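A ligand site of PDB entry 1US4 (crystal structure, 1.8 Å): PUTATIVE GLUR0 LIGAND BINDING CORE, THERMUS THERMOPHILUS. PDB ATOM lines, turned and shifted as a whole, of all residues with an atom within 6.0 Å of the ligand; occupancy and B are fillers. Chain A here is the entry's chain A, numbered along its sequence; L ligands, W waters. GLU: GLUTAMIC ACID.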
ATOM      1  N   SER A  25      16.460 -30.600 -21.819  1.00  0.00           N
ATOM      2  CA  SER A  25      15.581 -31.044 -22.902  1.00  0.00           C
ATOM      3  C   SER A  25      14.128 -30.626 -22.718  1.00  0.00           C
ATOM      4  O   SER A  25      13.803 -29.446 -22.831  1.00  0.00           O
ATOM      5  CB  SER A  25      15.694 -32.568 -23.062  1.00  0.00           C
ATOM      6  OG  SER A  25      15.324 -33.262 -21.885  1.00  0.00           O
ATOM      7  N   GLY A  26      13.247 -31.592 -22.460  1.00  0.00           N
ATOM      8  CA  GLY A  26      11.837 -31.283 -22.269  1.00  0.00           C
ATOM      9  C   GLY A  26      11.120 -32.451 -21.612  1.00  0.00           C
ATOM     10  O   GLY A  26      11.754 -33.238 -20.917  1.00  0.00           O
ATOM     11  N   SER A  27       9.805 -32.570 -21.816  1.00  0.00           N
ATOM     12  CA  SER A  27       9.051 -33.680 -21.242  1.00  0.00           C
ATOM     13  C   SER A  27       9.629 -34.997 -21.737  1.00  0.00           C
ATOM     14  O   SER A  27      10.111 -35.075 -22.865  1.00  0.00           O
ATOM     15  CB  SER A  27       7.568 -33.593 -21.627  1.00  0.00           C
ATOM     16  OG  SER A  27       6.928 -32.486 -21.011  1.00  0.00           O
ATOM     17  N   GLY A  30       8.322 -36.053 -25.102  1.00  0.00           N
ATOM     18  CA  GLY A  30       8.429 -35.099 -26.192  1.00  0.00           C
ATOM     19  C   GLY A  30       9.510 -35.610 -27.125  1.00  0.00           C
ATOM     20  O   GLY A  30       9.786 -36.816 -27.162  1.00  0.00           O
ATOM     21  N   VAL A  31      10.140 -34.715 -27.880  1.00  0.00           N
ATOM     22  CA  VAL A  31      11.209 -35.122 -28.801  1.00  0.00           C
ATOM     23  C   VAL A  31      12.571 -34.658 -28.289  1.00  0.00           C
ATOM     24  O   VAL A  31      13.581 -35.331 -28.509  1.00  0.00           O
ATOM     25  CB  VAL A  31      10.936 -34.570 -30.224  1.00  0.00           C
ATOM     26  CG1 VAL A  31      12.087 -34.941 -31.155  1.00  0.00           C
ATOM     27  CG2 VAL A  31       9.642 -35.168 -30.763  1.00  0.00           C
ATOM     28  N   TYR A  32      12.603 -33.518 -27.608  1.00  0.00           N
ATOM     29  CA  TYR A  32      13.870 -33.025 -27.058  1.00  0.00           C
ATOM     30  C   TYR A  32      14.535 -34.078 -26.167  1.00  0.00           C
ATOM     31  O   TYR A  32      15.739 -34.317 -26.274  1.00  0.00           O
ATOM     32  CB  TYR A  32      13.636 -31.797 -26.182  1.00  0.00           C
ATOM     33  CG  TYR A  32      13.425 -30.477 -26.888  1.00  0.00           C
ATOM     34  CD1 TYR A  32      13.410 -30.373 -28.282  1.00  0.00           C
ATOM     35  CD2 TYR A  32      13.236 -29.314 -26.137  1.00  0.00           C
ATOM     36  CE1 TYR A  32      13.210 -29.130 -28.909  1.00  0.00           C
ATOM     37  CE2 TYR A  32      13.040 -28.091 -26.737  1.00  0.00           C
ATOM     38  CZ  TYR A  32      13.020 -27.992 -28.119  1.00  0.00           C
ATOM     39  OH  TYR A  32      12.785 -26.762 -28.684  1.00  0.00           O
ATOM     40  N   PHE A  33      13.755 -34.685 -25.273  1.00  0.00           N
ATOM     41  CA  PHE A  33      14.304 -35.671 -24.351  1.00  0.00           C
ATOM     42  C   PHE A  33      14.983 -36.875 -24.999  1.00  0.00           C
ATOM     43  O   PHE A  33      16.126 -37.188 -24.680  1.00  0.00           O
ATOM     44  CB  PHE A  33      13.221 -36.145 -23.369  1.00  0.00           C
ATOM     45  CG  PHE A  33      13.744 -37.046 -22.293  1.00  0.00           C
ATOM     46  CD1 PHE A  33      14.570 -36.538 -21.298  1.00  0.00           C
ATOM     47  CD2 PHE A  33      13.453 -38.401 -22.292  1.00  0.00           C
ATOM     48  CE1 PHE A  33      15.099 -37.374 -20.308  1.00  0.00           C
ATOM     49  CE2 PHE A  33      13.982 -39.244 -21.314  1.00  0.00           C
ATOM     50  CZ  PHE A  33      14.805 -38.735 -20.328  1.00  0.00           C
ATOM     51  N   GLY A  58      11.044 -28.275 -18.353  1.00  0.00           N
ATOM     52  CA  GLY A  58       9.819 -27.688 -18.882  1.00  0.00           C
ATOM     53  C   GLY A  58       9.956 -27.215 -20.322  1.00  0.00           C
ATOM     54  O   GLY A  58       8.955 -26.887 -20.957  1.00  0.00           O
ATOM     55  N   GLY A  59      11.181 -27.166 -20.832  1.00  0.00           N
ATOM     56  CA  GLY A  59      11.360 -26.720 -22.206  1.00  0.00           C
ATOM     57  C   GLY A  59      12.320 -25.574 -22.435  1.00  0.00           C
ATOM     58  O   GLY A  59      13.153 -25.252 -21.586  1.00  0.00           O
ATOM     59  N   SER A  60      12.174 -24.927 -23.583  1.00  0.00           N
ATOM     60  CA  SER A  60      13.051 -23.829 -24.008  1.00  0.00           C
ATOM     61  C   SER A  60      13.388 -22.729 -23.010  1.00  0.00           C
ATOM     62  O   SER A  60      14.566 -22.409 -22.828  1.00  0.00           O
ATOM     63  CB  SER A  60      12.500 -23.188 -25.286  1.00  0.00           C
ATOM     64  OG  SER A  60      12.523 -24.108 -26.363  1.00  0.00           O
ATOM     65  N   VAL A  61      12.377 -22.130 -22.395  1.00  0.00           N
ATOM     66  CA  VAL A  61      12.647 -21.039 -21.451  1.00  0.00           C
ATOM     67  C   VAL A  61      13.431 -21.540 -20.248  1.00  0.00           C
ATOM     68  O   VAL A  61      14.437 -20.948 -19.868  1.00  0.00           O
ATOM     69  CB  VAL A  61      11.331 -20.363 -20.996  1.00  0.00           C
ATOM     70  CG1 VAL A  61      11.620 -19.316 -19.927  1.00  0.00           C
ATOM     71  CG2 VAL A  61      10.655 -19.700 -22.183  1.00  0.00           C
ATOM     72  N   LEU A  76      18.357 -28.085 -25.646  1.00  0.00           N
ATOM     73  CA  LEU A  76      17.625 -27.954 -26.895  1.00  0.00           C
ATOM     74  C   LEU A  76      16.693 -26.771 -26.658  1.00  0.00           C
ATOM     75  O   LEU A  76      16.268 -26.526 -25.529  1.00  0.00           O
ATOM     76  CB  LEU A  76      16.781 -29.201 -27.209  1.00  0.00           C
ATOM     77  CG  LEU A  76      17.504 -30.452 -27.731  1.00  0.00           C
ATOM     78  CD1 LEU A  76      18.127 -30.162 -29.084  1.00  0.00           C
ATOM     79  CD2 LEU A  76      18.552 -30.902 -26.738  1.00  0.00           C
ATOM     80  N   ALA A  77      16.402 -26.011 -27.712  1.00  0.00           N
ATOM     81  CA  ALA A  77      15.526 -24.859 -27.586  1.00  0.00           C
ATOM     82  C   ALA A  77      15.033 -24.413 -28.954  1.00  0.00           C
ATOM     83  O   ALA A  77      15.679 -24.676 -29.970  1.00  0.00           O
ATOM     84  CB  ALA A  77      16.267 -23.705 -26.911  1.00  0.00           C
ATOM     85  N   GLN A  78      13.881 -23.754 -28.968  1.00  0.00           N
ATOM     86  CA  GLN A  78      13.302 -23.256 -30.220  1.00  0.00           C
ATOM     87  C   GLN A  78      14.094 -22.052 -30.692  1.00  0.00           C
ATOM     88  O   GLN A  78      14.593 -21.267 -29.875  1.00  0.00           O
ATOM     89  CB  GLN A  78      11.839 -22.867 -29.996  1.00  0.00           C
ATOM     90  CG  GLN A  78      10.983 -24.002 -29.467  1.00  0.00           C
ATOM     91  CD  GLN A  78       9.547 -23.591 -29.140  1.00  0.00           C
ATOM     92  OE1 GLN A  78       8.789 -24.364 -28.565  1.00  0.00           O
ATOM     93  NE2 GLN A  78       9.177 -22.356 -29.506  1.00  0.00           N
ATOM     94  N   ILE A  81      12.578 -18.697 -29.385  1.00  0.00           N
ATOM     95  CA  ILE A  81      12.855 -18.442 -27.980  1.00  0.00           C
ATOM     96  C   ILE A  81      14.320 -18.063 -27.767  1.00  0.00           C
ATOM     97  O   ILE A  81      14.637 -17.173 -26.975  1.00  0.00           O
ATOM     98  CB  ILE A  81      12.506 -19.669 -27.106  1.00  0.00           C
ATOM     99  CG1 ILE A  81      11.040 -20.084 -27.347  1.00  0.00           C
ATOM    100  CG2 ILE A  81      12.725 -19.349 -25.626  1.00  0.00           C
ATOM    101  CD1 ILE A  81      10.008 -18.988 -27.038  1.00  0.00           C
ATOM    102  N   TYR A 109      15.557 -29.782 -36.554  1.00  0.00           N
ATOM    103  CA  TYR A 109      14.351 -30.200 -37.260  1.00  0.00           C
ATOM    104  C   TYR A 109      13.221 -29.224 -36.941  1.00  0.00           C
ATOM    105  O   TYR A 109      13.313 -28.435 -36.015  1.00  0.00           O
ATOM    106  CB  TYR A 109      13.965 -31.625 -36.821  1.00  0.00           C
ATOM    107  CG  TYR A 109      13.695 -31.750 -35.332  1.00  0.00           C
ATOM    108  CD1 TYR A 109      12.479 -31.348 -34.782  1.00  0.00           C
ATOM    109  CD2 TYR A 109      14.689 -32.218 -34.453  1.00  0.00           C
ATOM    110  CE1 TYR A 109      12.252 -31.401 -33.391  1.00  0.00           C
ATOM    111  CE2 TYR A 109      14.477 -32.261 -33.077  1.00  0.00           C
ATOM    112  CZ  TYR A 109      13.259 -31.849 -32.556  1.00  0.00           C
ATOM    113  OH  TYR A 109      13.051 -31.863 -31.197  1.00  0.00           O
ATOM    114  N   GLU A 111       9.761 -27.784 -35.492  1.00  0.00           N
ATOM    115  CA  GLU A 111       8.896 -28.012 -34.345  1.00  0.00           C
ATOM    116  C   GLU A 111       7.563 -27.412 -34.737  1.00  0.00           C
ATOM    117  O   GLU A 111       7.438 -26.200 -34.945  1.00  0.00           O
ATOM    118  CB  GLU A 111       9.460 -27.328 -33.107  1.00  0.00           C
ATOM    119  CG  GLU A 111      10.727 -27.983 -32.627  1.00  0.00           C
ATOM    120  CD  GLU A 111      11.032 -27.633 -31.203  1.00  0.00           C
ATOM    121  OE1 GLU A 111      11.834 -26.700 -30.978  1.00  0.00           O
ATOM    122  OE2 GLU A 111      10.457 -28.283 -30.302  1.00  0.00           O
ATOM    123  N   GLY A 140       7.797 -22.868 -18.086  1.00  0.00           N
ATOM    124  CA  GLY A 140       9.111 -22.644 -18.679  1.00  0.00           C
ATOM    125  C   GLY A 140       9.242 -23.238 -20.064  1.00  0.00           C
ATOM    126  O   GLY A 140      10.354 -23.465 -20.556  1.00  0.00           O
ATOM    127  N   SER A 141       8.112 -23.476 -20.709  1.00  0.00           N
ATOM    128  CA  SER A 141       8.112 -24.059 -22.047  1.00  0.00           C
ATOM    129  C   SER A 141       8.102 -23.019 -23.166  1.00  0.00           C
ATOM    130  O   SER A 141       7.722 -21.864 -22.963  1.00  0.00           O
ATOM    131  CB  SER A 141       6.888 -24.948 -22.236  1.00  0.00           C
ATOM    132  OG  SER A 141       5.697 -24.159 -22.243  1.00  0.00           O
ATOM    133  N   GLY A 142       8.545 -23.444 -24.347  1.00  0.00           N
ATOM    134  CA  GLY A 142       8.514 -22.561 -25.489  1.00  0.00           C
ATOM    135  C   GLY A 142       7.071 -22.600 -25.955  1.00  0.00           C
ATOM    136  O   GLY A 142       6.532 -21.609 -26.471  1.00  0.00           O
ATOM    137  N   THR A 143       6.449 -23.758 -25.759  1.00  0.00           N
ATOM    138  CA  THR A 143       5.049 -23.985 -26.148  1.00  0.00           C
ATOM    139  C   THR A 143       4.131 -22.885 -25.609  1.00  0.00           C
ATOM    140  O   THR A 143       3.301 -22.353 -26.349  1.00  0.00           O
ATOM    141  CB  THR A 143       4.537 -25.358 -25.611  1.00  0.00           C
ATOM    142  OG1 THR A 143       5.299 -26.415 -26.195  1.00  0.00           O
ATOM    143  CG2 THR A 143       3.063 -25.543 -25.944  1.00  0.00           C
ATOM    144  N   GLU A 144       4.266 -22.544 -24.331  1.00  0.00           N
ATOM    145  CA  GLU A 144       3.410 -21.518 -23.731  1.00  0.00           C
ATOM    146  C   GLU A 144       3.527 -20.183 -24.461  1.00  0.00           C
ATOM    147  O   GLU A 144       2.536 -19.473 -24.639  1.00  0.00           O
ATOM    148  CB  GLU A 144       3.744 -21.297 -22.256  1.00  0.00           C
ATOM    149  CG  GLU A 144       2.706 -20.432 -21.560  1.00  0.00           C
ATOM    150  CD  GLU A 144       3.084 -20.050 -20.144  1.00  0.00           C
ATOM    151  OE1 GLU A 144       3.729 -20.863 -19.458  1.00  0.00           O
ATOM    152  OE2 GLU A 144       2.702 -18.937 -19.712  1.00  0.00           O
ATOM    153  N   TYR A 186       1.188 -27.946 -27.995  1.00  0.00           N
ATOM    154  CA  TYR A 186       2.515 -28.536 -27.879  1.00  0.00           C
ATOM    155  C   TYR A 186       3.325 -28.167 -29.109  1.00  0.00           C
ATOM    156  O   TYR A 186       2.990 -28.575 -30.222  1.00  0.00           O
ATOM    157  CB  TYR A 186       2.432 -30.065 -27.746  1.00  0.00           C
ATOM    158  CG  TYR A 186       3.662 -30.721 -27.103  1.00  0.00           C
ATOM    159  CD1 TYR A 186       4.668 -29.950 -26.517  1.00  0.00           C
ATOM    160  CD2 TYR A 186       3.755 -32.113 -27.005  1.00  0.00           C
ATOM    161  CE1 TYR A 186       5.744 -30.554 -25.843  1.00  0.00           C
ATOM    162  CE2 TYR A 186       4.822 -32.721 -26.329  1.00  0.00           C
ATOM    163  CZ  TYR A 186       5.806 -31.933 -25.753  1.00  0.00           C
ATOM    164  OH  TYR A 186       6.833 -32.535 -25.041  1.00  0.00           O
ATOM    165  N   THR A 187       4.354 -27.346 -28.919  1.00  0.00           N
ATOM    166  CA  THR A 187       5.225 -26.970 -30.029  1.00  0.00           C
ATOM    167  C   THR A 187       6.263 -28.075 -29.965  1.00  0.00           C
ATOM    168  O   THR A 187       7.135 -28.081 -29.095  1.00  0.00           O
ATOM    169  CB  THR A 187       5.896 -25.612 -29.784  1.00  0.00           C
ATOM    170  OG1 THR A 187       4.876 -24.601 -29.679  1.00  0.00           O
ATOM    171  CG2 THR A 187       6.822 -25.263 -30.951  1.00  0.00           C
ATOM    172  N   VAL A 188       6.181 -29.028 -30.894  1.00  0.00           N
ATOM    173  CA  VAL A 188       7.074 -30.165 -30.840  1.00  0.00           C
ATOM    174  C   VAL A 188       7.268 -30.809 -32.203  1.00  0.00           C
ATOM    175  O   VAL A 188       6.475 -30.611 -33.117  1.00  0.00           O
ATOM    176  CB  VAL A 188       6.506 -31.205 -29.844  1.00  0.00           C
ATOM    177  CG1 VAL A 188       5.148 -31.688 -30.328  1.00  0.00           C
ATOM    178  CG2 VAL A 188       7.467 -32.369 -29.658  1.00  0.00           C
ATOM    179  N   GLY A 189       8.339 -31.588 -32.335  1.00  0.00           N
ATOM    180  CA  GLY A 189       8.600 -32.265 -33.587  1.00  0.00           C
ATOM    181  C   GLY A 189       7.523 -33.300 -33.834  1.00  0.00           C
ATOM    182  O   GLY A 189       6.890 -33.792 -32.904  1.00  0.00           O
HETATM  183  N   GLU L   1       9.881 -26.916 -28.077  1.00  0.00           N
HETATM  184  CA  GLU L   1       9.153 -27.280 -26.831  1.00  0.00           C
HETATM  185  C   GLU L   1       9.392 -26.254 -25.727  1.00  0.00           C
HETATM  186  O   GLU L   1      10.433 -25.554 -25.769  1.00  0.00           O
HETATM  187  CB  GLU L   1       9.611 -28.670 -26.364  1.00  0.00           C
HETATM  188  CG  GLU L   1       9.362 -29.773 -27.383  1.00  0.00           C
HETATM  189  CD  GLU L   1       9.976 -31.099 -26.989  1.00  0.00           C
HETATM  190  OE1 GLU L   1      10.184 -31.317 -25.770  1.00  0.00           O
HETATM  191  OE2 GLU L   1      10.240 -31.926 -27.884  1.00  0.00           O
HETATM  192  OXT GLU L   1       8.532 -26.150 -24.830  1.00  0.00           O
HETATM  193  O   HOH W   1       8.507 -30.894 -23.755  1.00  0.00           O
HETATM  194  O   HOH W   2      10.600 -30.961 -30.479  1.00  0.00           O
HETATM  195  O   HOH W   3       7.843 -28.337 -22.991  1.00  0.00           O
HETATM  196  O   HOH W   4      11.164 -33.651 -24.814  1.00  0.00           O
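Residues that only touch the ligand: Ser 141 (3.3 Å), Val 188 (3.3 Å), Tyr 186 (3.6 Å), Gly 59 (3.8 Å), Gly 30 (3.8 Å), Gly 26 (3.9 Å) and Gly 58 (3.97 Å). Hydrophobic or aromatic side chains that line the ligand: Val 31, Tyr 32 and Val 188.
An oxygen (OE2) of the ligand sits at hydrogen-bond distance from the backbone NH (N) of Val 31 (2.8 Å). N of the ligand is in hydrogen-bond range of OH of Tyr 32. The backbone NH (N) of Tyr 32 lies within hydrogen-bond range of an oxygen (OE2) of the ligand, at 2.9 Å. The backbone NH (N) of Ser 60 sits at hydrogen-bond distance from an oxygen (O) of the ligand, 2.9 Å away. The side-chain amide oxygen (OE1) of Gln 78 lies within hydrogen-bond range of a nitrogen (N) of the ligand (2.8 Å). O of Thr 187 sits close to N of the ligand, at 3.2 Å. N of Thr 143 sits at hydrogen-bond distance from OXT of the ligand. The side-chain carboxylate of Glu 111 is in salt-bridge range of a nitrogen (N) of the ligand. N of Gly 142 sits at hydrogen-bond distance from OXT of the ligand (2.7 Å). An oxygen (O) of the ligand lies within hydrogen-bond range of the side-chain hydroxyl of Ser 60, 2.6 Å away.
The side-chain hydroxyl (OG) of Ser 141 lies within hydrogen-bond range of the backbone NH (N) of Glu 144. OG of Ser 60 is in hydrogen-bond range of N of Gln 78. The side-chain carboxylate (OE1) of Glu 111 is in hydrogen-bond range of the side-chain hydroxyl (OH) of Tyr 32 (2.5 Å). N of Thr 187 sits at hydrogen-bond distance from OG1 of Thr 143 (3.0 Å). The backbone NH (N) of Gln 78 lies within hydrogen-bond range of the side-chain hydroxyl (OH) of Tyr 32.
Water W1 lies within hydrogen-bond range of an oxygen (OE1) of the ligand (2.7 Å), the side-chain hydroxyl of Tyr 186 (2.7 Å) and the backbone NH of Ser 27 (2.9 Å). Water W2 lies within hydrogen-bond range of OE2 of Glu 111 (2.7 Å), OH of Tyr 109 (2.7 Å), OE2 of the ligand (2.8 Å) and N of Gly 189 (3.0 Å). Water W3 lies within hydrogen-bond range of the backbone carbonyl oxygen of Gly 58 (2.7 Å) and an oxygen (OXT) of the ligand (2.9 Å).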
